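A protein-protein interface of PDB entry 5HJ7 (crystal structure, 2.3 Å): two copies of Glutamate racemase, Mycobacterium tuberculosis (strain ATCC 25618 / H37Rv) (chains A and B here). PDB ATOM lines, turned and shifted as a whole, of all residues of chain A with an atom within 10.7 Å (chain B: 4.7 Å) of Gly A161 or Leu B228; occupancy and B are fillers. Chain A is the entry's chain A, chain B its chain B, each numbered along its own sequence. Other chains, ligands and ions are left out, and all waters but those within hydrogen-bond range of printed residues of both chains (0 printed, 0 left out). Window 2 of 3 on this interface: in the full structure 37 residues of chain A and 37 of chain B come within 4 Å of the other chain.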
ATOM      1  N   PHE A 150      13.713  -2.377  28.457  1.00  0.00           N
ATOM      2  CA  PHE A 150      12.323  -1.919  28.468  1.00  0.00           C
ATOM      3  C   PHE A 150      12.159  -0.631  29.267  1.00  0.00           C
ATOM      4  O   PHE A 150      11.465   0.297  28.821  1.00  0.00           O
ATOM      5  CB  PHE A 150      11.406  -3.007  29.031  1.00  0.00           C
ATOM      6  CG  PHE A 150      10.905  -3.990  27.995  1.00  0.00           C
ATOM      7  CD1 PHE A 150      11.269  -3.858  26.657  1.00  0.00           C
ATOM      8  CD2 PHE A 150      10.070  -5.047  28.359  1.00  0.00           C
ATOM      9  CE1 PHE A 150      10.823  -4.755  25.701  1.00  0.00           C
ATOM     10  CE2 PHE A 150       9.622  -5.953  27.400  1.00  0.00           C
ATOM     11  CZ  PHE A 150      10.007  -5.798  26.056  1.00  0.00           C
ATOM     12  N   PHE A 153      13.244   2.462  27.345  1.00  0.00           N
ATOM     13  CA  PHE A 153      12.331   2.767  26.249  1.00  0.00           C
ATOM     14  C   PHE A 153      11.037   3.394  26.767  1.00  0.00           C
ATOM     15  O   PHE A 153      10.543   4.372  26.193  1.00  0.00           O
ATOM     16  CB  PHE A 153      12.054   1.499  25.433  1.00  0.00           C
ATOM     17  CG  PHE A 153      13.065   1.256  24.329  1.00  0.00           C
ATOM     18  CD1 PHE A 153      14.335   0.776  24.621  1.00  0.00           C
ATOM     19  CD2 PHE A 153      12.756   1.537  23.004  1.00  0.00           C
ATOM     20  CE1 PHE A 153      15.285   0.576  23.602  1.00  0.00           C
ATOM     21  CE2 PHE A 153      13.692   1.330  21.985  1.00  0.00           C
ATOM     22  CZ  PHE A 153      14.960   0.849  22.289  1.00  0.00           C
ATOM     23  N   GLY A 157       9.699   7.253  26.197  1.00  0.00           N
ATOM     24  CA  GLY A 157       8.450   7.280  25.463  1.00  0.00           C
ATOM     25  C   GLY A 157       8.456   6.601  24.109  1.00  0.00           C
ATOM     26  O   GLY A 157       7.722   7.029  23.209  1.00  0.00           O
ATOM     27  N   VAL A 158       9.240   5.539  23.941  1.00  0.00           N
ATOM     28  CA  VAL A 158       9.301   4.797  22.684  1.00  0.00           C
ATOM     29  C   VAL A 158       8.727   3.396  22.884  1.00  0.00           C
ATOM     30  O   VAL A 158       9.471   2.432  23.124  1.00  0.00           O
ATOM     31  CB  VAL A 158      10.750   4.740  22.171  1.00  0.00           C
ATOM     32  CG1 VAL A 158      10.827   4.051  20.802  1.00  0.00           C
ATOM     33  CG2 VAL A 158      11.327   6.145  22.132  1.00  0.00           C
ATOM     34  N   THR A 159       7.403   3.262  22.776  1.00  0.00           N
ATOM     35  CA  THR A 159       6.731   2.028  23.173  1.00  0.00           C
ATOM     36  C   THR A 159       5.863   1.419  22.073  1.00  0.00           C
ATOM     37  O   THR A 159       5.091   0.491  22.349  1.00  0.00           O
ATOM     38  CB  THR A 159       5.879   2.281  24.415  1.00  0.00           C
ATOM     39  OG1 THR A 159       4.880   3.261  24.103  1.00  0.00           O
ATOM     40  CG2 THR A 159       6.759   2.775  25.593  1.00  0.00           C
ATOM     41  N   SER A 160       5.970   1.910  20.841  1.00  0.00           N
ATOM     42  CA  SER A 160       5.332   1.292  19.684  1.00  0.00           C
ATOM     43  C   SER A 160       6.253   1.488  18.489  1.00  0.00           C
ATOM     44  O   SER A 160       7.197   2.287  18.540  1.00  0.00           O
ATOM     45  CB  SER A 160       3.939   1.884  19.400  1.00  0.00           C
ATOM     46  OG  SER A 160       4.043   3.271  19.092  1.00  0.00           O
ATOM     47  N   GLY A 161       5.972   0.765  17.402  1.00  0.00           N
ATOM     48  CA  GLY A 161       6.794   0.848  16.207  1.00  0.00           C
ATOM     49  C   GLY A 161       7.793  -0.297  16.095  1.00  0.00           C
ATOM     50  O   GLY A 161       7.891  -1.180  16.957  1.00  0.00           O
ATOM     51  N   ARG A 162       8.568  -0.248  15.000  1.00  0.00           N
ATOM     52  CA  ARG A 162       9.359  -1.407  14.586  1.00  0.00           C
ATOM     53  C   ARG A 162      10.596  -1.610  15.460  1.00  0.00           C
ATOM     54  O   ARG A 162      10.965  -2.754  15.752  1.00  0.00           O
ATOM     55  CB  ARG A 162       9.760  -1.269  13.117  1.00  0.00           C
ATOM     56  CG  ARG A 162       8.660  -1.707  12.154  1.00  0.00           C
ATOM     57  CD  ARG A 162       8.954  -1.286  10.708  1.00  0.00           C
ATOM     58  NE  ARG A 162       7.819  -0.577  10.118  1.00  0.00           N
ATOM     59  CZ  ARG A 162       7.785   0.737   9.898  1.00  0.00           C
ATOM     60  NH1 ARG A 162       8.834   1.498  10.199  1.00  0.00           N
ATOM     61  NH2 ARG A 162       6.700   1.291   9.372  1.00  0.00           N
ATOM     62  N   GLN A 163      11.262  -0.526  15.873  1.00  0.00           N
ATOM     63  CA  GLN A 163      12.466  -0.670  16.684  1.00  0.00           C
ATOM     64  C   GLN A 163      12.150  -1.402  17.982  1.00  0.00           C
ATOM     65  O   GLN A 163      12.725  -2.459  18.275  1.00  0.00           O
ATOM     66  CB  GLN A 163      13.094   0.699  16.977  1.00  0.00           C
ATOM     67  CG  GLN A 163      14.465   0.577  17.667  1.00  0.00           C
ATOM     68  CD  GLN A 163      14.974   1.856  18.335  1.00  0.00           C
ATOM     69  OE1 GLN A 163      14.208   2.755  18.692  1.00  0.00           O
ATOM     70  NE2 GLN A 163      16.283   1.927  18.520  1.00  0.00           N
ATOM     71  N   VAL A 164      11.206  -0.865  18.762  1.00  0.00           N
ATOM     72  CA  VAL A 164      10.901  -1.468  20.054  1.00  0.00           C
ATOM     73  C   VAL A 164      10.165  -2.793  19.872  1.00  0.00           C
ATOM     74  O   VAL A 164      10.272  -3.686  20.722  1.00  0.00           O
ATOM     75  CB  VAL A 164      10.116  -0.485  20.946  1.00  0.00           C
ATOM     76  CG1 VAL A 164       8.701  -0.274  20.422  1.00  0.00           C
ATOM     77  CG2 VAL A 164      10.103  -0.973  22.407  1.00  0.00           C
ATOM     78  N   LEU A 165       9.433  -2.971  18.767  1.00  0.00           N
ATOM     79  CA  LEU A 165       8.788  -4.268  18.561  1.00  0.00           C
ATOM     80  C   LEU A 165       9.828  -5.361  18.370  1.00  0.00           C
ATOM     81  O   LEU A 165       9.695  -6.454  18.930  1.00  0.00           O
ATOM     82  CB  LEU A 165       7.830  -4.236  17.372  1.00  0.00           C
ATOM     83  CG  LEU A 165       7.212  -5.604  17.030  1.00  0.00           C
ATOM     84  CD1 LEU A 165       6.344  -6.138  18.166  1.00  0.00           C
ATOM     85  CD2 LEU A 165       6.406  -5.564  15.732  1.00  0.00           C
ATOM     86  N   GLY A 166      10.879  -5.076  17.596  1.00  0.00           N
ATOM     87  CA  GLY A 166      11.955  -6.046  17.445  1.00  0.00           C
ATOM     88  C   GLY A 166      12.666  -6.330  18.752  1.00  0.00           C
ATOM     89  O   GLY A 166      13.041  -7.470  19.031  1.00  0.00           O
ATOM     90  N   LEU A 167      12.854  -5.297  19.574  1.00  0.00           N
ATOM     91  CA  LEU A 167      13.446  -5.506  20.891  1.00  0.00           C
ATOM     92  C   LEU A 167      12.628  -6.499  21.716  1.00  0.00           C
ATOM     93  O   LEU A 167      13.184  -7.416  22.341  1.00  0.00           O
ATOM     94  CB  LEU A 167      13.560  -4.164  21.607  1.00  0.00           C
ATOM     95  CG  LEU A 167      14.077  -4.151  23.040  1.00  0.00           C
ATOM     96  CD1 LEU A 167      15.530  -4.609  23.111  1.00  0.00           C
ATOM     97  CD2 LEU A 167      13.918  -2.750  23.606  1.00  0.00           C
ATOM     98  N   ALA A 168      11.302  -6.337  21.714  1.00  0.00           N
ATOM     99  CA  ALA A 168      10.442  -7.210  22.500  1.00  0.00           C
ATOM    100  C   ALA A 168      10.393  -8.615  21.919  1.00  0.00           C
ATOM    101  O   ALA A 168      10.400  -9.596  22.669  1.00  0.00           O
ATOM    102  CB  ALA A 168       9.036  -6.615  22.604  1.00  0.00           C
ATOM    103  N   GLN A 169      10.351  -8.743  20.589  1.00  0.00           N
ATOM    104  CA  GLN A 169      10.374 -10.081  19.995  1.00  0.00           C
ATOM    105  C   GLN A 169      11.623 -10.852  20.417  1.00  0.00           C
ATOM    106  O   GLN A 169      11.551 -12.058  20.697  1.00  0.00           O
ATOM    107  CB  GLN A 169      10.293  -9.995  18.470  1.00  0.00           C
ATOM    108  CG  GLN A 169       8.977  -9.462  17.925  1.00  0.00           C
ATOM    109  CD  GLN A 169       7.814 -10.433  18.122  1.00  0.00           C
ATOM    110  OE1 GLN A 169       7.979 -11.537  18.662  1.00  0.00           O
ATOM    111  NE2 GLN A 169       6.628 -10.022  17.675  1.00  0.00           N
ATOM    112  N   LEU A 192       3.013   0.312  30.572  1.00  0.00           N
ATOM    113  CA  LEU A 192       3.057   1.223  29.434  1.00  0.00           C
ATOM    114  C   LEU A 192       3.492   0.522  28.154  1.00  0.00           C
ATOM    115  O   LEU A 192       3.533   1.154  27.082  1.00  0.00           O
ATOM    116  CB  LEU A 192       3.977   2.415  29.733  1.00  0.00           C
ATOM    117  CG  LEU A 192       3.360   3.506  30.622  1.00  0.00           C
ATOM    118  CD1 LEU A 192       3.187   3.030  32.038  1.00  0.00           C
ATOM    119  CD2 LEU A 192       4.213   4.773  30.608  1.00  0.00           C
ATOM    120  N   LEU A 193       3.789  -0.771  28.246  1.00  0.00           N
ATOM    121  CA  LEU A 193       4.148  -1.597  27.109  1.00  0.00           C
ATOM    122  C   LEU A 193       3.138  -2.704  26.865  1.00  0.00           C
ATOM    123  O   LEU A 193       3.413  -3.606  26.065  1.00  0.00           O
ATOM    124  CB  LEU A 193       5.529  -2.218  27.325  1.00  0.00           C
ATOM    125  CG  LEU A 193       6.716  -1.303  27.065  1.00  0.00           C
ATOM    126  CD1 LEU A 193       8.007  -1.960  27.542  1.00  0.00           C
ATOM    127  CD2 LEU A 193       6.778  -0.972  25.575  1.00  0.00           C
ATOM    128  N   GLY A 195       0.236  -2.879  25.342  1.00  0.00           N
ATOM    129  CA  GLY A 195      -0.162  -2.997  23.943  1.00  0.00           C
ATOM    130  C   GLY A 195       0.920  -3.631  23.084  1.00  0.00           C
ATOM    131  O   GLY A 195       0.667  -4.572  22.326  1.00  0.00           O
ATOM    132  N   LEU A 196       2.150  -3.140  23.218  1.00  0.00           N
ATOM    133  CA  LEU A 196       3.269  -3.677  22.457  1.00  0.00           C
ATOM    134  C   LEU A 196       3.519  -5.151  22.796  1.00  0.00           C
ATOM    135  O   LEU A 196       3.667  -5.992  21.895  1.00  0.00           O
ATOM    136  CB  LEU A 196       4.499  -2.811  22.722  1.00  0.00           C
ATOM    137  CG  LEU A 196       5.750  -2.929  21.843  1.00  0.00           C
ATOM    138  CD1 LEU A 196       6.636  -4.017  22.371  1.00  0.00           C
ATOM    139  CD2 LEU A 196       5.425  -3.153  20.369  1.00  0.00           C
ATOM    140  N   ILE A 197       3.540  -5.486  24.089  1.00  0.00           N
ATOM    141  CA  ILE A 197       3.788  -6.865  24.503  1.00  0.00           C
ATOM    142  C   ILE A 197       2.656  -7.782  24.054  1.00  0.00           C
ATOM    143  O   ILE A 197       2.894  -8.946  23.707  1.00  0.00           O
ATOM    144  CB  ILE A 197       4.006  -6.933  26.026  1.00  0.00           C
ATOM    145  CG1 ILE A 197       5.238  -6.108  26.417  1.00  0.00           C
ATOM    146  CG2 ILE A 197       4.157  -8.377  26.471  1.00  0.00           C
ATOM    147  CD1 ILE A 197       5.435  -5.903  27.919  1.00  0.00           C
ATOM    148  N   LEU A 199       0.766  -7.441  21.348  1.00  0.00           N
ATOM    149  CA  LEU A 199       0.985  -7.658  19.924  1.00  0.00           C
ATOM    150  C   LEU A 199       2.061  -8.708  19.687  1.00  0.00           C
ATOM    151  O   LEU A 199       1.940  -9.542  18.784  1.00  0.00           O
ATOM    152  CB  LEU A 199       1.372  -6.332  19.269  1.00  0.00           C
ATOM    153  CG  LEU A 199       1.683  -6.307  17.782  1.00  0.00           C
ATOM    154  CD1 LEU A 199       0.551  -6.962  17.021  1.00  0.00           C
ATOM    155  CD2 LEU A 199       1.846  -4.854  17.362  1.00  0.00           C
ATOM    156  N   ALA A 200       3.127  -8.678  20.483  1.00  0.00           N
ATOM    157  CA  ALA A 200       4.178  -9.676  20.339  1.00  0.00           C
ATOM    158  C   ALA A 200       3.662 -11.065  20.693  1.00  0.00           C
ATOM    159  O   ALA A 200       3.830 -12.007  19.915  1.00  0.00           O
ATOM    160  CB  ALA A 200       5.379  -9.306  21.207  1.00  0.00           C
ATOM    161  N   PRO B   6      -0.619   9.914   9.106  1.00  0.00           N
ATOM    162  CA  PRO B   6      -0.248   9.526  10.479  1.00  0.00           C
ATOM    163  C   PRO B   6      -0.221  10.705  11.440  1.00  0.00           C
ATOM    164  O   PRO B   6      -0.354  10.500  12.651  1.00  0.00           O
ATOM    165  CB  PRO B   6       1.151   8.906  10.314  1.00  0.00           C
ATOM    166  CG  PRO B   6       1.241   8.538   8.856  1.00  0.00           C
ATOM    167  CD  PRO B   6       0.429   9.573   8.129  1.00  0.00           C
ATOM    168  N   LEU B  30       0.326   5.184  23.920  1.00  0.00           N
ATOM    169  CA  LEU B  30       0.648   5.896  22.684  1.00  0.00           C
ATOM    170  C   LEU B  30       0.939   7.355  23.005  1.00  0.00           C
ATOM    171  O   LEU B  30       0.126   8.247  22.719  1.00  0.00           O
ATOM    172  CB  LEU B  30      -0.499   5.760  21.684  1.00  0.00           C
ATOM    173  CG  LEU B  30      -0.665   4.323  21.172  1.00  0.00           C
ATOM    174  CD1 LEU B  30      -2.071   4.091  20.624  1.00  0.00           C
ATOM    175  CD2 LEU B  30       0.403   3.974  20.114  1.00  0.00           C
ATOM    176  N   GLU B  33       0.697  10.156  20.003  1.00  0.00           N
ATOM    177  CA  GLU B  33      -0.512  10.330  19.208  1.00  0.00           C
ATOM    178  C   GLU B  33      -1.229  11.603  19.631  1.00  0.00           C
ATOM    179  O   GLU B  33      -1.416  11.848  20.828  1.00  0.00           O
ATOM    180  CB  GLU B  33      -1.449   9.127  19.356  1.00  0.00           C
ATOM    181  CG  GLU B  33      -0.890   7.823  18.810  1.00  0.00           C
ATOM    182  CD  GLU B  33      -0.774   7.828  17.289  1.00  0.00           C
ATOM    183  OE1 GLU B  33      -1.545   8.568  16.650  1.00  0.00           O
ATOM    184  OE2 GLU B  33       0.073   7.095  16.728  1.00  0.00           O
ATOM    185  N   LYS B  71      -7.896  10.312  12.000  1.00  0.00           N
ATOM    186  CA  LYS B  71      -7.542   9.098  11.273  1.00  0.00           C
ATOM    187  C   LYS B  71      -8.163   7.829  11.864  1.00  0.00           C
ATOM    188  O   LYS B  71      -8.129   6.775  11.218  1.00  0.00           O
ATOM    189  CB  LYS B  71      -6.023   8.945  11.244  1.00  0.00           C
ATOM    190  CG  LYS B  71      -5.413   8.603  12.611  1.00  0.00           C
ATOM    191  CD  LYS B  71      -3.886   8.578  12.542  1.00  0.00           C
ATOM    192  CE  LYS B  71      -3.259   8.385  13.893  1.00  0.00           C
ATOM    193  NZ  LYS B  71      -1.769   8.314  13.812  1.00  0.00           N
ATOM    194  N   LEU B 222      -3.446   0.634  14.698  1.00  0.00           N
ATOM    195  CA  LEU B 222      -2.548   1.628  14.120  1.00  0.00           C
ATOM    196  C   LEU B 222      -1.242   0.999  13.647  1.00  0.00           C
ATOM    197  O   LEU B 222      -0.675   1.428  12.637  1.00  0.00           O
ATOM    198  CB  LEU B 222      -2.268   2.748  15.126  1.00  0.00           C
ATOM    199  CG  LEU B 222      -3.450   3.637  15.535  1.00  0.00           C
ATOM    200  CD1 LEU B 222      -2.997   4.830  16.388  1.00  0.00           C
ATOM    201  CD2 LEU B 222      -4.228   4.102  14.303  1.00  0.00           C
ATOM    202  N   THR B 223      -0.740  -0.011  14.361  1.00  0.00           N
ATOM    203  CA  THR B 223       0.475  -0.687  13.903  1.00  0.00           C
ATOM    204  C   THR B 223       0.222  -1.431  12.598  1.00  0.00           C
ATOM    205  O   THR B 223       0.940  -1.234  11.610  1.00  0.00           O
ATOM    206  CB  THR B 223       1.002  -1.656  14.968  1.00  0.00           C
ATOM    207  OG1 THR B 223       1.429  -0.941  16.132  1.00  0.00           O
ATOM    208  CG2 THR B 223       2.173  -2.466  14.423  1.00  0.00           C
ATOM    209  N   ASP B 226      -0.063   0.655   9.713  1.00  0.00           N
ATOM    210  CA  ASP B 226       1.114   1.517   9.608  1.00  0.00           C
ATOM    211  C   ASP B 226       0.739   2.994   9.621  1.00  0.00           C
ATOM    212  O   ASP B 226       1.218   3.788   8.806  1.00  0.00           O
ATOM    213  CB  ASP B 226       1.945   1.182   8.367  1.00  0.00           C
ATOM    214  CG  ASP B 226       3.428   1.435   8.590  1.00  0.00           C
ATOM    215  OD1 ASP B 226       4.101   0.545   9.156  1.00  0.00           O
ATOM    216  OD2 ASP B 226       3.919   2.530   8.238  1.00  0.00           O
ATOM    217  N   LEU B 227      -0.100   3.370  10.595  1.00  0.00           N
ATOM    218  CA  LEU B 227      -0.568   4.744  10.764  1.00  0.00           C
ATOM    219  C   LEU B 227      -0.185   5.312  12.127  1.00  0.00           C
ATOM    220  O   LEU B 227      -0.917   6.118  12.696  1.00  0.00           O
ATOM    221  CB  LEU B 227      -2.080   4.821  10.562  1.00  0.00           C
ATOM    222  CG  LEU B 227      -2.634   5.901   9.625  1.00  0.00           C
ATOM    223  CD1 LEU B 227      -1.618   6.319   8.587  1.00  0.00           C
ATOM    224  CD2 LEU B 227      -3.896   5.390   8.936  1.00  0.00           C
ATOM    225  N   LEU B 228       0.960   4.898  12.657  1.00  0.00           N
ATOM    226  CA  LEU B 228       1.460   5.423  13.921  1.00  0.00           C
ATOM    227  C   LEU B 228       2.072   6.816  13.729  1.00  0.00           C
ATOM    228  O   LEU B 228       2.880   7.030  12.818  1.00  0.00           O
ATOM    229  CB  LEU B 228       2.492   4.447  14.501  1.00  0.00           C
ATOM    230  CG  LEU B 228       1.961   3.113  15.049  1.00  0.00           C
ATOM    231  CD1 LEU B 228       3.099   2.125  15.330  1.00  0.00           C
ATOM    232  CD2 LEU B 228       1.148   3.347  16.325  1.00  0.00           C
ATOM    233  N   ARG B 229       1.687   7.771  14.577  1.00  0.00           N
ATOM    234  CA  ARG B 229       2.342   9.076  14.535  1.00  0.00           C
ATOM    235  C   ARG B 229       3.807   8.919  14.943  1.00  0.00           C
ATOM    236  O   ARG B 229       4.094   8.300  15.975  1.00  0.00           O
ATOM    237  CB  ARG B 229       1.641  10.081  15.447  1.00  0.00           C
ATOM    238  CG  ARG B 229       2.074  11.523  15.182  1.00  0.00           C
ATOM    239  CD  ARG B 229       1.171  12.559  15.842  1.00  0.00           C
ATOM    240  NE  ARG B 229       1.663  13.927  15.682  1.00  0.00           N
ATOM    241  CZ  ARG B 229       2.571  14.493  16.468  1.00  0.00           C
ATOM    242  NH1 ARG B 229       3.095  13.816  17.489  1.00  0.00           N
ATOM    243  NH2 ARG B 229       2.946  15.747  16.244  1.00  0.00           N
ATOM    244  N   PRO B 230       4.755   9.447  14.172  1.00  0.00           N
ATOM    245  CA  PRO B 230       6.170   9.155  14.440  1.00  0.00           C
ATOM    246  C   PRO B 230       6.685   9.830  15.707  1.00  0.00           C
ATOM    247  O   PRO B 230       6.230  10.907  16.102  1.00  0.00           O
ATOM    248  CB  PRO B 230       6.886   9.702  13.199  1.00  0.00           C
ATOM    249  CG  PRO B 230       5.838   9.880  12.182  1.00  0.00           C
ATOM    250  CD  PRO B 230       4.581  10.191  12.917  1.00  0.00           C
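The side-chain carboxylate of Asp B226 lies within salt-bridge range of the guanidinium group of Arg A162 (2.7 Å).
Among the printed residues, merely in contact across the chains: Ser A160 with Leu B30 (3.8 Å), Gly A161 with Leu B228 (3.8 Å) and Leu A199 with Thr B223 (3.8 Å).
Thr A159 touches none of the printed residues of chain B.
Of the printed residues of chain B, Ser A160 touches Leu B30 (3.8 Å).
Printed residues of chain B within 4 Å of Gly A161: Leu B228 (3.8 Å).
Printed residues of chain B within 4 Å of Arg A162: Asp B226 (2.7 Å).
Leu A192 touches none of the printed residues of chain B.
Of the printed residues of chain B, Leu A199 touches Thr B223 (3.8 Å).
No residue of chain A comes within 4 Å of Pro B6.
Printed residues of chain A within 4 Å of Leu B30: Ser A160.
No residue of chain A comes within 4 Å of Leu B227.
Of the printed residues of chain A, Leu B228 touches Gly A161.
No residue of chain A comes within 4 Å of Pro B230.
The nearest printed residue of chain B that does not touch Arg A162 is Leu B228 (6.0 Å).
Printed residues of chain B that touch a printed residue of chain A: Leu B30, Thr B223, Asp B226 and Leu B228.
Hydrophobic or aromatic side chains of chain B within 4 Å of the printed part of chain A: Leu B30 and Leu B228.
Of the 22 printed residues of chain A, 4 touch a printed residue of chain B.
Hydrophobic or aromatic side chains of chain A that line the printed part of chain B: Leu A199.
Among the printed residues, 4 pairs touch across the chains.
Among the printed residues, Asp or Glu carboxylates within 4 Å of a Lys or Arg side-chain nitrogen of the other chain: Arg A162 with Asp B226 (2.7 Å).
No position is printed for both chains.
Of the 4 pairs that touch across the chains among the printed residues, none has its exchanged pair printed and touching as well.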
